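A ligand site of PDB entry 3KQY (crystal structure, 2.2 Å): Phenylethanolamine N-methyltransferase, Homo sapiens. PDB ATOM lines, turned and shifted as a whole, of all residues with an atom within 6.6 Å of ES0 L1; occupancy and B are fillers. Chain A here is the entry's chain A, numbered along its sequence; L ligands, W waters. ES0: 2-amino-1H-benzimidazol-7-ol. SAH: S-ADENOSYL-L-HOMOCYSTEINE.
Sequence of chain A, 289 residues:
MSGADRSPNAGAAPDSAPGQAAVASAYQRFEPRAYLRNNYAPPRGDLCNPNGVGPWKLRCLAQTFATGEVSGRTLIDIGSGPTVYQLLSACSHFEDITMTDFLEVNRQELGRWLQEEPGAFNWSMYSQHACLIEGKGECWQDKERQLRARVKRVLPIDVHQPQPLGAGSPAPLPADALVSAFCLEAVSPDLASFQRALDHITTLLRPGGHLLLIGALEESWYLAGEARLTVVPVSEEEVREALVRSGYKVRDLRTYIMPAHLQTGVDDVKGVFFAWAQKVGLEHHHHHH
The side-chain hydroxyl (OH) of Tyr 40 is in hydrogen-bond range of a nitrogen (NAF) of ES0 L1 (3.2 Å). A nitrogen (NAA) of ES0 L1 lies within hydrogen-bond range of the side-chain hydroxyl of Tyr 35 (2.8 Å). The guanidinium group (NH1) of Arg 44 lies within hydrogen-bond range of an oxygen (OAB) of ES0 L1 (3.2 Å). An oxygen (O) of SAH L2 is in hydrogen-bond range of the side-chain hydroxyl of Tyr 35 (2.5 Å). The side-chain hydroxyl (OH) of Tyr 40 lies within hydrogen-bond range of an oxygen (O) of SAH L2 (2.6 Å). The side-chain hydroxyl of Tyr 85 is in hydrogen-bond range of an oxygen (OXT) of SAH L2 (2.7 Å). O of Ala 181 sits at hydrogen-bond distance from N of SAH L2, at 2.8 Å.
Water W1 lies within hydrogen-bond range of NAA of ES0 L1 (2.7 Å) and OE2 of Glu 219 (3.2 Å).
The guanidinium group (NH1) of Arg 44 lies within hydrogen-bond range of the side-chain amide oxygen (OD1) of Asn 39 (3.1 Å). OD1 of Asp 267 sits close to N of Val 269 (3.2 Å). The guanidinium group (NE) of Arg 44 sits at hydrogen-bond distance from the backbone carbonyl oxygen (O) of Leu 262. The side-chain hydroxyl (OH) of Tyr 40 is in hydrogen-bond range of the side-chain hydroxyl (OH) of Tyr 85, 3.2 Å away. OD2 of Asp 267 lies within salt-bridge range of NH1 of Arg 44. ND2 of Asn 39 sits at hydrogen-bond distance from O of Tyr 35 (3.2 Å).
OD1 of Asn 39 touches NAG of ES0 L1, 3.7 Å away. Val 53 touches ES0 L1. NZ of Lys 57 touches CAE of ES0 L1, 3.0 Å away. Phe 182 touches ES0 L1 (CE1 to NAF, 3.4 Å). Met 258 touches ES0 L1. OD2 of Asp 267 touches OAB of ES0 L1, at 3.7 Å. CG1 of Val 269 touches OAB of ES0 L1, 3.4 Å away. Hydrophobic or aromatic side chains within 4 Å of ES0 L1: Tyr 35, Tyr 40, Val 53, Phe 182, Met 258 and Val 269. Ten residues have an atom within 4 Å of ES0 L1: Tyr 35, Asn 39, Tyr 40, Arg 44, Val 53, Lys 57, Phe 182, Met 258, Asp 267 and Val 269.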
ATOM      1  N   TYR A  35       1.977 -14.059  20.519  1.00  0.00           N
ATOM      2  CA  TYR A  35       1.702 -14.672  21.820  1.00  0.00           C
ATOM      3  C   TYR A  35       0.769 -13.792  22.650  1.00  0.00           C
ATOM      4  O   TYR A  35      -0.218 -14.269  23.210  1.00  0.00           O
ATOM      5  CB  TYR A  35       3.005 -14.937  22.569  1.00  0.00           C
ATOM      6  CG  TYR A  35       2.823 -15.427  23.989  1.00  0.00           C
ATOM      7  CD1 TYR A  35       2.388 -16.726  24.248  1.00  0.00           C
ATOM      8  CD2 TYR A  35       3.075 -14.586  25.065  1.00  0.00           C
ATOM      9  CE1 TYR A  35       2.218 -17.170  25.545  1.00  0.00           C
ATOM     10  CE2 TYR A  35       2.905 -15.029  26.362  1.00  0.00           C
ATOM     11  CZ  TYR A  35       2.474 -16.310  26.604  1.00  0.00           C
ATOM     12  OH  TYR A  35       2.299 -16.743  27.893  1.00  0.00           O
ATOM     13  N   ASN A  39      -3.239 -14.771  23.816  1.00  0.00           N
ATOM     14  CA  ASN A  39      -3.537 -15.045  25.214  1.00  0.00           C
ATOM     15  C   ASN A  39      -4.003 -13.841  26.024  1.00  0.00           C
ATOM     16  O   ASN A  39      -4.603 -13.996  27.089  1.00  0.00           O
ATOM     17  CB  ASN A  39      -2.311 -15.690  25.876  1.00  0.00           C
ATOM     18  CG  ASN A  39      -1.964 -17.029  25.259  1.00  0.00           C
ATOM     19  OD1 ASN A  39      -2.703 -17.994  25.403  1.00  0.00           O
ATOM     20  ND2 ASN A  39      -0.834 -17.087  24.558  1.00  0.00           N
ATOM     21  N   TYR A  40      -3.725 -12.639  25.531  1.00  0.00           N
ATOM     22  CA  TYR A  40      -4.002 -11.439  26.314  1.00  0.00           C
ATOM     23  C   TYR A  40      -4.789 -10.371  25.556  1.00  0.00           C
ATOM     24  O   TYR A  40      -4.915  -9.237  26.015  1.00  0.00           O
ATOM     25  CB  TYR A  40      -2.702 -10.878  26.889  1.00  0.00           C
ATOM     26  CG  TYR A  40      -2.021 -11.913  27.754  1.00  0.00           C
ATOM     27  CD1 TYR A  40      -0.951 -12.659  27.266  1.00  0.00           C
ATOM     28  CD2 TYR A  40      -2.479 -12.183  29.029  1.00  0.00           C
ATOM     29  CE1 TYR A  40      -0.343 -13.614  28.045  1.00  0.00           C
ATOM     30  CE2 TYR A  40      -1.872 -13.140  29.818  1.00  0.00           C
ATOM     31  CZ  TYR A  40      -0.810 -13.853  29.315  1.00  0.00           C
ATOM     32  OH  TYR A  40      -0.210 -14.802  30.104  1.00  0.00           O
ATOM     33  N   ARG A  44      -9.753 -14.137  25.616  1.00  0.00           N
ATOM     34  CA  ARG A  44      -9.096 -14.446  26.881  1.00  0.00           C
ATOM     35  C   ARG A  44      -8.701 -13.166  27.601  1.00  0.00           C
ATOM     36  O   ARG A  44      -8.620 -13.130  28.831  1.00  0.00           O
ATOM     37  CB  ARG A  44      -7.872 -15.343  26.660  1.00  0.00           C
ATOM     38  CG  ARG A  44      -8.239 -16.743  26.208  1.00  0.00           C
ATOM     39  CD  ARG A  44      -7.020 -17.607  26.003  1.00  0.00           C
ATOM     40  NE  ARG A  44      -7.397 -18.980  25.699  1.00  0.00           N
ATOM     41  CZ  ARG A  44      -6.541 -19.995  25.603  1.00  0.00           C
ATOM     42  NH1 ARG A  44      -5.242 -19.787  25.789  1.00  0.00           N
ATOM     43  NH2 ARG A  44      -6.975 -21.211  25.313  1.00  0.00           N
ATOM     44  N   VAL A  53     -10.673 -16.134  32.642  1.00  0.00           N
ATOM     45  CA  VAL A  53      -9.405 -16.598  33.223  1.00  0.00           C
ATOM     46  C   VAL A  53      -8.528 -15.437  33.671  1.00  0.00           C
ATOM     47  O   VAL A  53      -7.849 -15.515  34.698  1.00  0.00           O
ATOM     48  CB  VAL A  53      -8.646 -17.533  32.247  1.00  0.00           C
ATOM     49  CG1 VAL A  53      -8.370 -16.828  30.923  1.00  0.00           C
ATOM     50  CG2 VAL A  53      -7.352 -18.033  32.875  1.00  0.00           C
ATOM     51  N   GLY A  54      -8.528 -14.356  32.892  1.00  0.00           N
ATOM     52  CA  GLY A  54      -7.802 -13.152  33.268  1.00  0.00           C
ATOM     53  C   GLY A  54      -8.150 -12.653  34.661  1.00  0.00           C
ATOM     54  O   GLY A  54      -7.268 -12.504  35.502  1.00  0.00           O
ATOM     55  N   LYS A  57      -7.068 -15.142  37.380  1.00  0.00           N
ATOM     56  CA  LYS A  57      -5.649 -15.057  37.690  1.00  0.00           C
ATOM     57  C   LYS A  57      -5.312 -13.864  38.580  1.00  0.00           C
ATOM     58  O   LYS A  57      -4.650 -14.006  39.612  1.00  0.00           O
ATOM     59  CB  LYS A  57      -4.809 -14.974  36.415  1.00  0.00           C
ATOM     60  CG  LYS A  57      -4.757 -16.284  35.634  1.00  0.00           C
ATOM     61  CD  LYS A  57      -3.733 -16.203  34.526  1.00  0.00           C
ATOM     62  CE  LYS A  57      -4.236 -15.356  33.379  1.00  0.00           C
ATOM     63  NZ  LYS A  57      -3.215 -15.269  32.312  1.00  0.00           N
ATOM     64  N   TYR A  85       1.266  -8.429  33.694  1.00  0.00           N
ATOM     65  CA  TYR A  85       0.102  -8.593  34.562  1.00  0.00           C
ATOM     66  C   TYR A  85       0.464  -9.333  35.836  1.00  0.00           C
ATOM     67  O   TYR A  85      -0.084  -9.043  36.905  1.00  0.00           O
ATOM     68  CB  TYR A  85      -1.005  -9.357  33.836  1.00  0.00           C
ATOM     69  CG  TYR A  85      -0.691 -10.821  33.673  1.00  0.00           C
ATOM     70  CD1 TYR A  85      -1.101 -11.754  34.615  1.00  0.00           C
ATOM     71  CD2 TYR A  85       0.041 -11.283  32.583  1.00  0.00           C
ATOM     72  CE1 TYR A  85      -0.807 -13.096  34.474  1.00  0.00           C
ATOM     73  CE2 TYR A  85       0.345 -12.617  32.435  1.00  0.00           C
ATOM     74  CZ  TYR A  85      -0.082 -13.513  33.382  1.00  0.00           C
ATOM     75  OH  TYR A  85       0.220 -14.849  33.244  1.00  0.00           O
ATOM     76  N   ALA A 181       4.839 -17.555  35.740  1.00  0.00           N
ATOM     77  CA  ALA A 181       3.589 -17.930  35.085  1.00  0.00           C
ATOM     78  C   ALA A 181       3.797 -18.538  33.704  1.00  0.00           C
ATOM     79  O   ALA A 181       4.418 -17.930  32.825  1.00  0.00           O
ATOM     80  CB  ALA A 181       2.641 -16.727  35.012  1.00  0.00           C
ATOM     81  N   PHE A 182       3.266 -19.751  33.525  1.00  0.00           N
ATOM     82  CA  PHE A 182       3.288 -20.436  32.239  1.00  0.00           C
ATOM     83  C   PHE A 182       4.703 -20.656  31.675  1.00  0.00           C
ATOM     84  O   PHE A 182       4.890 -20.715  30.463  1.00  0.00           O
ATOM     85  CB  PHE A 182       2.423 -19.678  31.213  1.00  0.00           C
ATOM     86  CG  PHE A 182       1.000 -19.502  31.644  1.00  0.00           C
ATOM     87  CD1 PHE A 182       0.537 -18.273  32.100  1.00  0.00           C
ATOM     88  CD2 PHE A 182       0.113 -20.573  31.593  1.00  0.00           C
ATOM     89  CE1 PHE A 182      -0.784 -18.115  32.489  1.00  0.00           C
ATOM     90  CE2 PHE A 182      -1.209 -20.415  31.981  1.00  0.00           C
ATOM     91  CZ  PHE A 182      -1.657 -19.186  32.429  1.00  0.00           C
ATOM     92  N   GLU A 185       6.277 -25.658  32.849  1.00  0.00           N
ATOM     93  CA  GLU A 185       5.574 -26.647  32.047  1.00  0.00           C
ATOM     94  C   GLU A 185       5.723 -26.376  30.547  1.00  0.00           C
ATOM     95  O   GLU A 185       5.575 -27.278  29.720  1.00  0.00           O
ATOM     96  CB  GLU A 185       4.092 -26.741  32.446  1.00  0.00           C
ATOM     97  CG  GLU A 185       3.192 -25.650  31.853  1.00  0.00           C
ATOM     98  CD  GLU A 185       3.152 -24.374  32.681  1.00  0.00           C
ATOM     99  OE1 GLU A 185       3.890 -24.265  33.691  1.00  0.00           O
ATOM    100  OE2 GLU A 185       2.376 -23.464  32.314  1.00  0.00           O
ATOM    101  N   ALA A 216      -0.381 -23.749  32.904  1.00  0.00           N
ATOM    102  CA  ALA A 216      -1.353 -24.534  32.160  1.00  0.00           C
ATOM    103  C   ALA A 216      -1.478 -25.956  32.732  1.00  0.00           C
ATOM    104  O   ALA A 216      -0.479 -26.559  33.137  1.00  0.00           O
ATOM    105  CB  ALA A 216      -0.980 -24.575  30.688  1.00  0.00           C
ATOM    106  N   GLU A 219      -1.892 -29.408  29.372  1.00  0.00           N
ATOM    107  CA  GLU A 219      -1.633 -28.807  28.066  1.00  0.00           C
ATOM    108  C   GLU A 219      -0.436 -29.489  27.412  1.00  0.00           C
ATOM    109  O   GLU A 219       0.491 -29.898  28.105  1.00  0.00           O
ATOM    110  CB  GLU A 219      -1.359 -27.307  28.218  1.00  0.00           C
ATOM    111  CG  GLU A 219      -0.769 -26.661  26.984  1.00  0.00           C
ATOM    112  CD  GLU A 219      -0.651 -25.154  27.128  1.00  0.00           C
ATOM    113  OE1 GLU A 219      -1.658 -24.449  26.896  1.00  0.00           O
ATOM    114  OE2 GLU A 219       0.460 -24.674  27.448  1.00  0.00           O
ATOM    115  N   TYR A 222       1.142 -25.082  22.425  1.00  0.00           N
ATOM    116  CA  TYR A 222       0.557 -23.784  22.171  1.00  0.00           C
ATOM    117  C   TYR A 222       1.342 -23.078  21.077  1.00  0.00           C
ATOM    118  O   TYR A 222       2.547 -23.276  20.943  1.00  0.00           O
ATOM    119  CB  TYR A 222       0.509 -22.940  23.445  1.00  0.00           C
ATOM    120  CG  TYR A 222       1.832 -22.371  23.872  1.00  0.00           C
ATOM    121  CD1 TYR A 222       2.212 -21.088  23.480  1.00  0.00           C
ATOM    122  CD2 TYR A 222       2.703 -23.088  24.670  1.00  0.00           C
ATOM    123  CE1 TYR A 222       3.419 -20.553  23.864  1.00  0.00           C
ATOM    124  CE2 TYR A 222       3.922 -22.557  25.065  1.00  0.00           C
ATOM    125  CZ  TYR A 222       4.273 -21.295  24.655  1.00  0.00           C
ATOM    126  OH  TYR A 222       5.473 -20.753  25.040  1.00  0.00           O
ATOM    127  N   MET A 258     -10.976 -24.405  32.118  1.00  0.00           N
ATOM    128  CA  MET A 258     -11.114 -23.541  30.949  1.00  0.00           C
ATOM    129  C   MET A 258     -12.466 -23.751  30.262  1.00  0.00           C
ATOM    130  O   MET A 258     -12.764 -24.844  29.798  1.00  0.00           O
ATOM    131  CB  MET A 258      -9.951 -23.786  29.978  1.00  0.00           C
ATOM    132  CG  MET A 258      -9.587 -22.580  29.116  1.00  0.00           C
ATOM    133  SD  MET A 258      -8.894 -21.192  30.038  1.00  0.00           S
ATOM    134  CE  MET A 258      -7.151 -21.558  30.021  1.00  0.00           C
ATOM    135  N   LEU A 262     -13.456 -20.126  25.831  1.00  0.00           N
ATOM    136  CA  LEU A 262     -12.054 -19.727  25.914  1.00  0.00           C
ATOM    137  C   LEU A 262     -11.079 -20.721  25.282  1.00  0.00           C
ATOM    138  O   LEU A 262      -9.854 -20.563  25.408  1.00  0.00           O
ATOM    139  CB  LEU A 262     -11.660 -19.383  27.349  1.00  0.00           C
ATOM    140  CG  LEU A 262     -12.264 -18.062  27.837  1.00  0.00           C
ATOM    141  CD1 LEU A 262     -11.665 -17.663  29.166  1.00  0.00           C
ATOM    142  CD2 LEU A 262     -12.064 -16.964  26.799  1.00  0.00           C
ATOM    143  N   ASP A 267      -4.022 -23.248  21.473  1.00  0.00           N
ATOM    144  CA  ASP A 267      -3.422 -24.256  22.332  1.00  0.00           C
ATOM    145  C   ASP A 267      -4.454 -25.303  22.689  1.00  0.00           C
ATOM    146  O   ASP A 267      -5.543 -25.332  22.093  1.00  0.00           O
ATOM    147  CB  ASP A 267      -2.796 -23.626  23.587  1.00  0.00           C
ATOM    148  CG  ASP A 267      -3.817 -22.922  24.474  1.00  0.00           C
ATOM    149  OD1 ASP A 267      -4.968 -23.389  24.583  1.00  0.00           O
ATOM    150  OD2 ASP A 267      -3.445 -21.902  25.097  1.00  0.00           O
ATOM    151  N   VAL A 269      -4.847 -26.188  26.213  1.00  0.00           N
ATOM    152  CA  VAL A 269      -4.957 -26.081  27.660  1.00  0.00           C
ATOM    153  C   VAL A 269      -6.318 -26.582  28.116  1.00  0.00           C
ATOM    154  O   VAL A 269      -7.308 -26.459  27.399  1.00  0.00           O
ATOM    155  CB  VAL A 269      -4.747 -24.624  28.114  1.00  0.00           C
ATOM    156  CG1 VAL A 269      -5.819 -23.728  27.511  1.00  0.00           C
ATOM    157  CG2 VAL A 269      -4.740 -24.522  29.616  1.00  0.00           C
ATOM    158  N   GLY A 271      -7.018 -26.309  31.763  1.00  0.00           N
ATOM    159  CA  GLY A 271      -7.247 -25.534  32.959  1.00  0.00           C
ATOM    160  C   GLY A 271      -6.030 -24.692  33.263  1.00  0.00           C
ATOM    161  O   GLY A 271      -5.040 -24.741  32.535  1.00  0.00           O
ATOM    162  N   VAL A 272      -6.115 -23.906  34.325  1.00  0.00           N
ATOM    163  CA  VAL A 272      -4.986 -23.122  34.781  1.00  0.00           C
ATOM    164  C   VAL A 272      -4.885 -23.352  36.279  1.00  0.00           C
ATOM    165  O   VAL A 272      -5.907 -23.461  36.950  1.00  0.00           O
ATOM    166  CB  VAL A 272      -5.177 -21.615  34.474  1.00  0.00           C
ATOM    167  CG1 VAL A 272      -4.009 -20.810  35.011  1.00  0.00           C
ATOM    168  CG2 VAL A 272      -5.343 -21.385  32.979  1.00  0.00           C
HETATM  169  NAA ES0 L   1       0.659 -18.964  28.203  1.00  0.00           N
HETATM  170  OAB ES0 L   1      -4.275 -20.928  28.580  1.00  0.00           O
HETATM  171  CAC ES0 L   1      -4.709 -17.613  30.026  1.00  0.00           C
HETATM  172  CAD ES0 L   1      -4.995 -18.901  29.576  1.00  0.00           C
HETATM  173  CAE ES0 L   1      -3.418 -17.114  29.920  1.00  0.00           C
HETATM  174  NAF ES0 L   1      -1.115 -17.690  29.130  1.00  0.00           N
HETATM  175  NAG ES0 L   1      -1.578 -19.698  28.440  1.00  0.00           N
HETATM  176  CAH ES0 L   1      -0.615 -18.792  28.570  1.00  0.00           C
HETATM  177  CAI ES0 L   1      -3.995 -19.682  29.021  1.00  0.00           C
HETATM  178  CAJ ES0 L   1      -2.410 -17.901  29.355  1.00  0.00           C
HETATM  179  CAK ES0 L   1      -2.703 -19.183  28.915  1.00  0.00           C
HETATM  180  N   SAH L   2       5.176 -15.427  31.905  1.00  0.00           N
HETATM  181  CA  SAH L   2       4.523 -15.016  30.671  1.00  0.00           C
HETATM  182  CB  SAH L   2       5.114 -15.767  29.485  1.00  0.00           C
HETATM  183  CG  SAH L   2       4.961 -17.280  29.623  1.00  0.00           C
HETATM  184  SD  SAH L   2       5.287 -18.132  28.053  1.00  0.00           S
HETATM  185  C   SAH L   2       3.021 -15.235  30.786  1.00  0.00           C
HETATM  186  O   SAH L   2       2.382 -15.105  29.796  1.00  0.00           O
HETATM  187  OXT SAH L   2       2.527 -15.446  32.079  1.00  0.00           O
HETATM  188  C5' SAH L   2       6.808 -19.040  28.443  1.00  0.00           C
HETATM  189  C4' SAH L   2       8.111 -18.241  28.461  1.00  0.00           C
HETATM  190  O4' SAH L   2       9.170 -19.057  28.801  1.00  0.00           O
HETATM  191  C3' SAH L   2       8.482 -17.627  27.131  1.00  0.00           C
HETATM  192  O3' SAH L   2       8.608 -16.232  27.315  1.00  0.00           O
HETATM  193  C2' SAH L   2       9.704 -18.200  26.831  1.00  0.00           C
HETATM  194  O2' SAH L   2      10.566 -17.371  26.100  1.00  0.00           O
HETATM  195  C1' SAH L   2      10.253 -18.555  28.104  1.00  0.00           C
HETATM  196  N9  SAH L   2      11.344 -19.520  28.037  1.00  0.00           N
HETATM  197  C8  SAH L   2      11.625 -20.323  27.006  1.00  0.00           C
HETATM  198  N7  SAH L   2      12.708 -21.110  27.365  1.00  0.00           N
HETATM  199  C5  SAH L   2      13.072 -20.785  28.638  1.00  0.00           C
HETATM  200  C6  SAH L   2      14.058 -21.249  29.451  1.00  0.00           C
HETATM  201  N6  SAH L   2      14.943 -22.305  28.990  1.00  0.00           N
HETATM  202  N1  SAH L   2      14.207 -20.755  30.680  1.00  0.00           N
HETATM  203  C2  SAH L   2      13.373 -19.770  31.102  1.00  0.00           C
HETATM  204  N3  SAH L   2      12.394 -19.300  30.291  1.00  0.00           N
HETATM  205  C4  SAH L   2      12.249 -19.815  29.059  1.00  0.00           C
HETATM  206  O   HOH W   1       0.528 -21.476  27.156  1.00  0.00           O
